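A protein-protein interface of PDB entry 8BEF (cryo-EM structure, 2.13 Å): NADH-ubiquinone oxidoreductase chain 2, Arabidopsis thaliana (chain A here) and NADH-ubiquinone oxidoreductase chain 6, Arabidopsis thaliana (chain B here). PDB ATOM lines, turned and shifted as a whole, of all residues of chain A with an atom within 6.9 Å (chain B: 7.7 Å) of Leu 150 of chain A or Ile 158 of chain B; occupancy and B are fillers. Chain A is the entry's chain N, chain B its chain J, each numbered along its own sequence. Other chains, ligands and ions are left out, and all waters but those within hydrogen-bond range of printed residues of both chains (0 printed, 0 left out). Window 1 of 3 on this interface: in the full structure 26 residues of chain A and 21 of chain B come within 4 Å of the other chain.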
ATOM      1  N   GLY A 135      28.564  11.937 -29.962  1.00  0.00           N
ATOM      2  CA  GLY A 135      27.629  10.946 -29.457  1.00  0.00           C
ATOM      3  C   GLY A 135      27.996   9.529 -29.858  1.00  0.00           C
ATOM      4  O   GLY A 135      27.913   8.608 -29.050  1.00  0.00           O
ATOM      5  N   MET A 139      29.011   6.304 -27.793  1.00  0.00           N
ATOM      6  CA  MET A 139      28.301   5.047 -28.009  1.00  0.00           C
ATOM      7  C   MET A 139      29.270   3.873 -28.039  1.00  0.00           C
ATOM      8  O   MET A 139      29.017   2.830 -27.427  1.00  0.00           O
ATOM      9  CB  MET A 139      27.502   5.082 -29.314  1.00  0.00           C
ATOM     10  CG  MET A 139      26.239   5.921 -29.308  1.00  0.00           C
ATOM     11  SD  MET A 139      25.447   6.006 -30.924  1.00  0.00           S
ATOM     12  CE  MET A 139      25.122   4.271 -31.221  1.00  0.00           C
ATOM     13  N   ASP A 144      27.428   0.487 -20.114  1.00  0.00           N
ATOM     14  CA  ASP A 144      26.296   0.467 -19.202  1.00  0.00           C
ATOM     15  C   ASP A 144      25.070   0.876 -20.004  1.00  0.00           C
ATOM     16  O   ASP A 144      25.170   1.663 -20.948  1.00  0.00           O
ATOM     17  CB  ASP A 144      26.531   1.403 -18.004  1.00  0.00           C
ATOM     18  CG  ASP A 144      25.360   1.436 -17.030  1.00  0.00           C
ATOM     19  OD1 ASP A 144      25.553   1.030 -15.865  1.00  0.00           O
ATOM     20  OD2 ASP A 144      24.260   1.890 -17.407  1.00  0.00           O
ATOM     21  N   LEU A 145      23.913   0.328 -19.624  1.00  0.00           N
ATOM     22  CA  LEU A 145      22.692   0.595 -20.379  1.00  0.00           C
ATOM     23  C   LEU A 145      22.357   2.083 -20.381  1.00  0.00           C
ATOM     24  O   LEU A 145      21.886   2.620 -21.390  1.00  0.00           O
ATOM     25  CB  LEU A 145      21.532  -0.216 -19.808  1.00  0.00           C
ATOM     26  CG  LEU A 145      21.697  -1.735 -19.785  1.00  0.00           C
ATOM     27  CD1 LEU A 145      20.888  -2.336 -18.649  1.00  0.00           C
ATOM     28  CD2 LEU A 145      21.321  -2.351 -21.119  1.00  0.00           C
ATOM     29  N   ILE A 146      22.607   2.763 -19.260  1.00  0.00           N
ATOM     30  CA  ILE A 146      22.304   4.187 -19.150  1.00  0.00           C
ATOM     31  C   ILE A 146      23.160   4.997 -20.119  1.00  0.00           C
ATOM     32  O   ILE A 146      22.654   5.835 -20.878  1.00  0.00           O
ATOM     33  CB  ILE A 146      22.506   4.655 -17.698  1.00  0.00           C
ATOM     34  CG1 ILE A 146      21.538   3.921 -16.766  1.00  0.00           C
ATOM     35  CG2 ILE A 146      22.370   6.167 -17.598  1.00  0.00           C
ATOM     36  CD1 ILE A 146      21.863   4.076 -15.293  1.00  0.00           C
ATOM     37  N   ALA A 147      24.475   4.766 -20.090  1.00  0.00           N
ATOM     38  CA  ALA A 147      25.383   5.481 -20.983  1.00  0.00           C
ATOM     39  C   ALA A 147      25.051   5.192 -22.439  1.00  0.00           C
ATOM     40  O   ALA A 147      25.052   6.100 -23.283  1.00  0.00           O
ATOM     41  CB  ALA A 147      26.830   5.094 -20.674  1.00  0.00           C
ATOM     42  N   MET A 148      24.760   3.927 -22.745  1.00  0.00           N
ATOM     43  CA  MET A 148      24.400   3.544 -24.103  1.00  0.00           C
ATOM     44  C   MET A 148      23.164   4.299 -24.572  1.00  0.00           C
ATOM     45  O   MET A 148      23.147   4.862 -25.672  1.00  0.00           O
ATOM     46  CB  MET A 148      24.176   2.035 -24.170  1.00  0.00           C
ATOM     47  CG  MET A 148      23.809   1.507 -25.545  1.00  0.00           C
ATOM     48  SD  MET A 148      23.424  -0.254 -25.497  1.00  0.00           S
ATOM     49  CE  MET A 148      21.808  -0.233 -24.733  1.00  0.00           C
ATOM     50  N   TYR A 149      22.128   4.348 -23.728  1.00  0.00           N
ATOM     51  CA  TYR A 149      20.908   5.056 -24.099  1.00  0.00           C
ATOM     52  C   TYR A 149      21.170   6.540 -24.316  1.00  0.00           C
ATOM     53  O   TYR A 149      20.682   7.124 -25.289  1.00  0.00           O
ATOM     54  CB  TYR A 149      19.832   4.862 -23.032  1.00  0.00           C
ATOM     55  CG  TYR A 149      18.600   5.700 -23.284  1.00  0.00           C
ATOM     56  CD1 TYR A 149      17.681   5.341 -24.262  1.00  0.00           C
ATOM     57  CD2 TYR A 149      18.359   6.851 -22.551  1.00  0.00           C
ATOM     58  CE1 TYR A 149      16.555   6.103 -24.497  1.00  0.00           C
ATOM     59  CE2 TYR A 149      17.234   7.620 -22.782  1.00  0.00           C
ATOM     60  CZ  TYR A 149      16.338   7.240 -23.755  1.00  0.00           C
ATOM     61  OH  TYR A 149      15.218   7.997 -23.990  1.00  0.00           O
ATOM     62  N   LEU A 150      21.932   7.168 -23.419  1.00  0.00           N
ATOM     63  CA  LEU A 150      22.171   8.604 -23.544  1.00  0.00           C
ATOM     64  C   LEU A 150      22.913   8.926 -24.837  1.00  0.00           C
ATOM     65  O   LEU A 150      22.547   9.859 -25.566  1.00  0.00           O
ATOM     66  CB  LEU A 150      22.947   9.112 -22.331  1.00  0.00           C
ATOM     67  CG  LEU A 150      22.179   9.174 -21.009  1.00  0.00           C
ATOM     68  CD1 LEU A 150      23.036   9.805 -19.936  1.00  0.00           C
ATOM     69  CD2 LEU A 150      20.864   9.932 -21.166  1.00  0.00           C
ATOM     70  N   ALA A 151      23.960   8.156 -25.139  1.00  0.00           N
ATOM     71  CA  ALA A 151      24.731   8.403 -26.354  1.00  0.00           C
ATOM     72  C   ALA A 151      23.887   8.160 -27.604  1.00  0.00           C
ATOM     73  O   ALA A 151      23.935   8.947 -28.565  1.00  0.00           O
ATOM     74  CB  ALA A 151      25.986   7.534 -26.345  1.00  0.00           C
ATOM     75  N   ILE A 152      23.085   7.090 -27.595  1.00  0.00           N
ATOM     76  CA  ILE A 152      22.182   6.817 -28.709  1.00  0.00           C
ATOM     77  C   ILE A 152      21.221   7.980 -28.916  1.00  0.00           C
ATOM     78  O   ILE A 152      20.967   8.395 -30.050  1.00  0.00           O
ATOM     79  CB  ILE A 152      21.428   5.493 -28.473  1.00  0.00           C
ATOM     80  CG1 ILE A 152      22.374   4.297 -28.610  1.00  0.00           C
ATOM     81  CG2 ILE A 152      20.260   5.355 -29.432  1.00  0.00           C
ATOM     82  CD1 ILE A 152      21.695   2.968 -28.393  1.00  0.00           C
ATOM     83  N   GLU A 153      20.680   8.527 -27.825  1.00  0.00           N
ATOM     84  CA  GLU A 153      19.724   9.625 -27.944  1.00  0.00           C
ATOM     85  C   GLU A 153      20.379  10.888 -28.492  1.00  0.00           C
ATOM     86  O   GLU A 153      19.775  11.598 -29.303  1.00  0.00           O
ATOM     87  CB  GLU A 153      19.074   9.910 -26.592  1.00  0.00           C
ATOM     88  CG  GLU A 153      18.120   8.833 -26.116  1.00  0.00           C
ATOM     89  CD  GLU A 153      17.196   8.330 -27.209  1.00  0.00           C
ATOM     90  OE1 GLU A 153      16.198   9.013 -27.508  1.00  0.00           O
ATOM     91  OE2 GLU A 153      17.467   7.244 -27.765  1.00  0.00           O
ATOM     92  N   LEU A 154      21.593  11.204 -28.038  1.00  0.00           N
ATOM     93  CA  LEU A 154      22.297  12.368 -28.577  1.00  0.00           C
ATOM     94  C   LEU A 154      22.474  12.238 -30.088  1.00  0.00           C
ATOM     95  O   LEU A 154      22.130  13.152 -30.863  1.00  0.00           O
ATOM     96  CB  LEU A 154      23.650  12.522 -27.880  1.00  0.00           C
ATOM     97  CG  LEU A 154      24.666  13.526 -28.436  1.00  0.00           C
ATOM     98  CD1 LEU A 154      24.057  14.908 -28.592  1.00  0.00           C
ATOM     99  CD2 LEU A 154      25.903  13.585 -27.554  1.00  0.00           C
ATOM    100  N   GLN A 155      22.984  11.082 -30.518  1.00  0.00           N
ATOM    101  CA  GLN A 155      23.128  10.788 -31.939  1.00  0.00           C
ATOM    102  C   GLN A 155      21.801  10.937 -32.686  1.00  0.00           C
ATOM    103  O   GLN A 155      21.728  11.586 -33.741  1.00  0.00           O
ATOM    104  CB  GLN A 155      23.701   9.375 -32.072  1.00  0.00           C
ATOM    105  CG  GLN A 155      24.052   8.926 -33.455  1.00  0.00           C
ATOM    106  CD  GLN A 155      23.220   7.740 -33.867  1.00  0.00           C
ATOM    107  OE1 GLN A 155      21.997   7.761 -33.754  1.00  0.00           O
ATOM    108  NE2 GLN A 155      23.880   6.689 -34.347  1.00  0.00           N
ATOM    109  N   SER A 156      20.733  10.361 -32.130  1.00  0.00           N
ATOM    110  CA  SER A 156      19.438  10.363 -32.801  1.00  0.00           C
ATOM    111  C   SER A 156      18.880  11.773 -32.946  1.00  0.00           C
ATOM    112  O   SER A 156      18.320  12.115 -33.991  1.00  0.00           O
ATOM    113  CB  SER A 156      18.452   9.479 -32.040  1.00  0.00           C
ATOM    114  OG  SER A 156      18.625   8.114 -32.370  1.00  0.00           O
ATOM    115  N   LEU A 157      18.987  12.590 -31.899  1.00  0.00           N
ATOM    116  CA  LEU A 157      18.448  13.943 -31.965  1.00  0.00           C
ATOM    117  C   LEU A 157      19.191  14.773 -33.007  1.00  0.00           C
ATOM    118  O   LEU A 157      18.570  15.524 -33.777  1.00  0.00           O
ATOM    119  CB  LEU A 157      18.510  14.598 -30.585  1.00  0.00           C
ATOM    120  CG  LEU A 157      17.612  13.919 -29.544  1.00  0.00           C
ATOM    121  CD1 LEU A 157      17.880  14.428 -28.136  1.00  0.00           C
ATOM    122  CD2 LEU A 157      16.146  14.061 -29.908  1.00  0.00           C
ATOM    123  N   TYR B 148      28.898  10.038 -11.346  1.00  0.00           N
ATOM    124  CA  TYR B 148      28.266   9.823 -12.641  1.00  0.00           C
ATOM    125  C   TYR B 148      28.186  11.127 -13.425  1.00  0.00           C
ATOM    126  O   TYR B 148      27.228  11.377 -14.158  1.00  0.00           O
ATOM    127  CB  TYR B 148      26.892   9.183 -12.456  1.00  0.00           C
ATOM    128  CG  TYR B 148      26.995   7.832 -11.789  1.00  0.00           C
ATOM    129  CD1 TYR B 148      27.292   6.698 -12.530  1.00  0.00           C
ATOM    130  CD2 TYR B 148      26.833   7.694 -10.416  1.00  0.00           C
ATOM    131  CE1 TYR B 148      27.410   5.463 -11.931  1.00  0.00           C
ATOM    132  CE2 TYR B 148      26.945   6.456  -9.805  1.00  0.00           C
ATOM    133  CZ  TYR B 148      27.235   5.345 -10.572  1.00  0.00           C
ATOM    134  OH  TYR B 148      27.350   4.108  -9.984  1.00  0.00           O
ATOM    135  N   VAL B 150      29.802  12.245 -16.020  1.00  0.00           N
ATOM    136  CA  VAL B 150      29.880  12.179 -17.480  1.00  0.00           C
ATOM    137  C   VAL B 150      28.486  12.106 -18.096  1.00  0.00           C
ATOM    138  O   VAL B 150      28.206  12.762 -19.107  1.00  0.00           O
ATOM    139  CB  VAL B 150      30.760  10.992 -17.918  1.00  0.00           C
ATOM    140  CG1 VAL B 150      30.790  10.886 -19.435  1.00  0.00           C
ATOM    141  CG2 VAL B 150      32.166  11.147 -17.367  1.00  0.00           C
ATOM    142  N   TRP B 151      27.598  11.298 -17.511  1.00  0.00           N
ATOM    143  CA  TRP B 151      26.235  11.183 -18.028  1.00  0.00           C
ATOM    144  C   TRP B 151      25.481  12.505 -17.895  1.00  0.00           C
ATOM    145  O   TRP B 151      24.729  12.901 -18.796  1.00  0.00           O
ATOM    146  CB  TRP B 151      25.504  10.053 -17.299  1.00  0.00           C
ATOM    147  CG  TRP B 151      26.204   8.720 -17.382  1.00  0.00           C
ATOM    148  CD1 TRP B 151      27.198   8.368 -18.249  1.00  0.00           C
ATOM    149  CD2 TRP B 151      25.935   7.555 -16.590  1.00  0.00           C
ATOM    150  NE1 TRP B 151      27.574   7.065 -18.036  1.00  0.00           N
ATOM    151  CE2 TRP B 151      26.814   6.544 -17.024  1.00  0.00           C
ATOM    152  CE3 TRP B 151      25.043   7.275 -15.553  1.00  0.00           C
ATOM    153  CZ2 TRP B 151      26.824   5.272 -16.458  1.00  0.00           C
ATOM    154  CZ3 TRP B 151      25.053   6.009 -14.992  1.00  0.00           C
ATOM    155  CH2 TRP B 151      25.938   5.024 -15.447  1.00  0.00           C
ATOM    156  N   PHE B 152      25.675  13.190 -16.768  1.00  0.00           N
ATOM    157  CA  PHE B 152      25.171  14.544 -16.554  1.00  0.00           C
ATOM    158  C   PHE B 152      25.589  15.483 -17.692  1.00  0.00           C
ATOM    159  O   PHE B 152      24.756  16.179 -18.297  1.00  0.00           O
ATOM    160  CB  PHE B 152      25.706  14.999 -15.188  1.00  0.00           C
ATOM    161  CG  PHE B 152      25.401  16.413 -14.810  1.00  0.00           C
ATOM    162  CD1 PHE B 152      24.107  16.898 -14.815  1.00  0.00           C
ATOM    163  CD2 PHE B 152      26.423  17.245 -14.374  1.00  0.00           C
ATOM    164  CE1 PHE B 152      23.846  18.197 -14.432  1.00  0.00           C
ATOM    165  CE2 PHE B 152      26.164  18.545 -13.992  1.00  0.00           C
ATOM    166  CZ  PHE B 152      24.876  19.019 -14.020  1.00  0.00           C
ATOM    167  N   LEU B 153      26.881  15.482 -18.025  1.00  0.00           N
ATOM    168  CA  LEU B 153      27.369  16.371 -19.077  1.00  0.00           C
ATOM    169  C   LEU B 153      26.840  15.972 -20.457  1.00  0.00           C
ATOM    170  O   LEU B 153      26.540  16.838 -21.292  1.00  0.00           O
ATOM    171  CB  LEU B 153      28.895  16.398 -19.058  1.00  0.00           C
ATOM    172  CG  LEU B 153      29.512  17.016 -17.802  1.00  0.00           C
ATOM    173  CD1 LEU B 153      31.023  17.093 -17.926  1.00  0.00           C
ATOM    174  CD2 LEU B 153      28.919  18.398 -17.519  1.00  0.00           C
ATOM    175  N   VAL B 154      26.715  14.670 -20.723  1.00  0.00           N
ATOM    176  CA  VAL B 154      26.142  14.244 -22.000  1.00  0.00           C
ATOM    177  C   VAL B 154      24.696  14.722 -22.122  1.00  0.00           C
ATOM    178  O   VAL B 154      24.245  15.126 -23.203  1.00  0.00           O
ATOM    179  CB  VAL B 154      26.257  12.717 -22.167  1.00  0.00           C
ATOM    180  CG1 VAL B 154      25.506  12.259 -23.412  1.00  0.00           C
ATOM    181  CG2 VAL B 154      27.719  12.305 -22.260  1.00  0.00           C
ATOM    182  N   SER B 155      23.952  14.694 -21.014  1.00  0.00           N
ATOM    183  CA  SER B 155      22.600  15.247 -21.029  1.00  0.00           C
ATOM    184  C   SER B 155      22.621  16.735 -21.365  1.00  0.00           C
ATOM    185  O   SER B 155      21.745  17.233 -22.092  1.00  0.00           O
ATOM    186  CB  SER B 155      21.918  15.009 -19.682  1.00  0.00           C
ATOM    187  OG  SER B 155      22.229  16.042 -18.766  1.00  0.00           O
ATOM    188  N   SER B 156      23.607  17.464 -20.832  1.00  0.00           N
ATOM    189  CA  SER B 156      23.766  18.864 -21.230  1.00  0.00           C
ATOM    190  C   SER B 156      23.962  18.995 -22.738  1.00  0.00           C
ATOM    191  O   SER B 156      23.402  19.900 -23.372  1.00  0.00           O
ATOM    192  CB  SER B 156      24.942  19.505 -20.495  1.00  0.00           C
ATOM    193  OG  SER B 156      26.175  19.186 -21.104  1.00  0.00           O
ATOM    194  N   LEU B 157      24.765  18.108 -23.326  1.00  0.00           N
ATOM    195  CA  LEU B 157      24.953  18.140 -24.777  1.00  0.00           C
ATOM    196  C   LEU B 157      23.633  17.914 -25.508  1.00  0.00           C
ATOM    197  O   LEU B 157      23.359  18.549 -26.538  1.00  0.00           O
ATOM    198  CB  LEU B 157      25.986  17.097 -25.202  1.00  0.00           C
ATOM    199  CG  LEU B 157      27.455  17.419 -24.927  1.00  0.00           C
ATOM    200  CD1 LEU B 157      28.353  16.342 -25.521  1.00  0.00           C
ATOM    201  CD2 LEU B 157      27.817  18.795 -25.477  1.00  0.00           C
ATOM    202  N   ILE B 158      22.807  17.007 -24.987  1.00  0.00           N
ATOM    203  CA  ILE B 158      21.497  16.746 -25.581  1.00  0.00           C
ATOM    204  C   ILE B 158      20.639  18.013 -25.566  1.00  0.00           C
ATOM    205  O   ILE B 158      19.989  18.364 -26.564  1.00  0.00           O
ATOM    206  CB  ILE B 158      20.818  15.574 -24.843  1.00  0.00           C
ATOM    207  CG1 ILE B 158      21.418  14.236 -25.289  1.00  0.00           C
ATOM    208  CG2 ILE B 158      19.319  15.586 -25.046  1.00  0.00           C
ATOM    209  CD1 ILE B 158      21.107  13.084 -24.355  1.00  0.00           C
ATOM    210  N   LEU B 159      20.649  18.732 -24.442  1.00  0.00           N
ATOM    211  CA  LEU B 159      19.878  19.974 -24.364  1.00  0.00           C
ATOM    212  C   LEU B 159      20.410  21.027 -25.335  1.00  0.00           C
ATOM    213  O   LEU B 159      19.631  21.766 -25.953  1.00  0.00           O
ATOM    214  CB  LEU B 159      19.873  20.508 -22.934  1.00  0.00           C
ATOM    215  CG  LEU B 159      19.121  19.634 -21.926  1.00  0.00           C
ATOM    216  CD1 LEU B 159      19.228  20.215 -20.530  1.00  0.00           C
ATOM    217  CD2 LEU B 159      17.661  19.446 -22.336  1.00  0.00           C
ATOM    218  N   LEU B 160      21.736  21.109 -25.482  1.00  0.00           N
ATOM    219  CA  LEU B 160      22.316  22.040 -26.449  1.00  0.00           C
ATOM    220  C   LEU B 160      21.843  21.725 -27.864  1.00  0.00           C
ATOM    221  O   LEU B 160      21.525  22.638 -28.643  1.00  0.00           O
ATOM    222  CB  LEU B 160      23.844  21.996 -26.371  1.00  0.00           C
ATOM    223  CG  LEU B 160      24.609  22.808 -27.421  1.00  0.00           C
ATOM    224  CD1 LEU B 160      24.308  24.278 -27.270  1.00  0.00           C
ATOM    225  CD2 LEU B 160      26.107  22.560 -27.321  1.00  0.00           C
ATOM    226  N   VAL B 161      21.797  20.436 -28.212  1.00  0.00           N
ATOM    227  CA  VAL B 161      21.269  20.039 -29.514  1.00  0.00           C
ATOM    228  C   VAL B 161      19.830  20.512 -29.665  1.00  0.00           C
ATOM    229  O   VAL B 161      19.434  21.004 -30.727  1.00  0.00           O
ATOM    230  CB  VAL B 161      21.384  18.514 -29.709  1.00  0.00           C
ATOM    231  CG1 VAL B 161      20.609  18.079 -30.947  1.00  0.00           C
ATOM    232  CG2 VAL B 161      22.836  18.104 -29.824  1.00  0.00           C
ATOM    233  N   ALA B 162      19.022  20.357 -28.612  1.00  0.00           N
ATOM    234  CA  ALA B 162      17.633  20.810 -28.686  1.00  0.00           C
ATOM    235  C   ALA B 162      17.553  22.303 -28.990  1.00  0.00           C
ATOM    236  O   ALA B 162      16.773  22.732 -29.848  1.00  0.00           O
ATOM    237  CB  ALA B 162      16.896  20.489 -27.386  1.00  0.00           C
ATOM    238  N   MET B 163      18.364  23.108 -28.299  1.00  0.00           N
ATOM    239  CA  MET B 163      18.346  24.556 -28.521  1.00  0.00           C
ATOM    240  C   MET B 163      18.726  24.899 -29.960  1.00  0.00           C
ATOM    241  O   MET B 163      18.024  25.666 -30.646  1.00  0.00           O
ATOM    242  CB  MET B 163      19.293  25.245 -27.535  1.00  0.00           C
ATOM    243  CG  MET B 163      19.152  24.739 -26.112  1.00  0.00           C
ATOM    244  SD  MET B 163      20.405  25.279 -24.933  1.00  0.00           S
ATOM    245  CE  MET B 163      20.182  27.045 -24.946  1.00  0.00           C
ATOM    246  N   ILE B 164      19.828  24.319 -30.440  1.00  0.00           N
ATOM    247  CA  ILE B 164      20.293  24.609 -31.794  1.00  0.00           C
ATOM    248  C   ILE B 164      19.240  24.206 -32.816  1.00  0.00           C
ATOM    249  O   ILE B 164      18.930  24.964 -33.744  1.00  0.00           O
ATOM    250  CB  ILE B 164      21.636  23.908 -32.067  1.00  0.00           C
ATOM    251  CG1 ILE B 164      22.766  24.578 -31.285  1.00  0.00           C
ATOM    252  CG2 ILE B 164      21.938  23.902 -33.561  1.00  0.00           C
ATOM    253  CD1 ILE B 164      24.079  23.831 -31.364  1.00  0.00           C
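Leu 150 of chain A touches just these residues of chain B: Trp 151 (3.6 Å) and Ile 158 (3.7 Å).
Ile 158 of chain B touches just these residues of chain A: Leu 150, Leu 154 and Leu 157.
Of the printed residues of chain A, Trp 151 of chain B touches Asp 144, Ile 146, Ala 147 and Leu 150.
Of the printed residues of chain B, Ala 147 of chain A touches Trp 151 (3.4 Å).
Printed residues of chain B within 4 Å of Asp 144 of chain A: Trp 151 (3.96 Å).
Of the printed residues of chain B, Leu 154 of chain A touches Ile 158 (3.8 Å) and Val 161 (3.6 Å).
Of the printed residues of chain A, Val 161 of chain B touches Leu 154.
Ser 156 of chain A touches none of the printed residues of chain B.
The nearest residue of chain B that does not touch Leu 150 of chain A is Val 154 of chain B (4.2 Å).
The nearest residue of chain A that does not touch Ile 158 of chain B is Glu 153 of chain A (4.4 Å).
The nearest printed residue of chain B that does not touch Ala 147 of chain A is Val 154 of chain B (6.2 Å).
Among the printed residues, pairs that only touch across the chains: Ala 147 of chain A with Trp 151 of chain B (3.4 Å), Ile 146 of chain A with Trp 151 of chain B (3.5 Å), Leu 157 of chain A with Ile 158 of chain B (3.6 Å), Leu 150 of chain A with Trp 151 of chain B (3.6 Å), Leu 154 of chain A with Val 161 of chain B (3.6 Å), Leu 150 of chain A with Ile 158 of chain B (3.7 Å), Leu 154 of chain A with Ile 158 of chain B (3.8 Å) and Asp 144 of chain A with Trp 151 of chain B (3.96 Å).
Of the 16 printed residues of chain A, 6 touch a printed residue of chain B.
Hydrophobic or aromatic side chains of chain A within 4 Å of the printed part of chain B: Ile 146, Ala 147, Leu 150, Leu 154 and Leu 157.
Of the 16 printed residues of chain B, 3 touch a printed residue of chain A.
Hydrophobic or aromatic side chains of chain B within 4 Å of the printed part of chain A: Trp 151, Ile 158 and Val 161.
The side-chain carboxylate of Asp 144 of chain A sits at hydrogen-bond distance from the backbone NH of Ile 146 of chain A.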
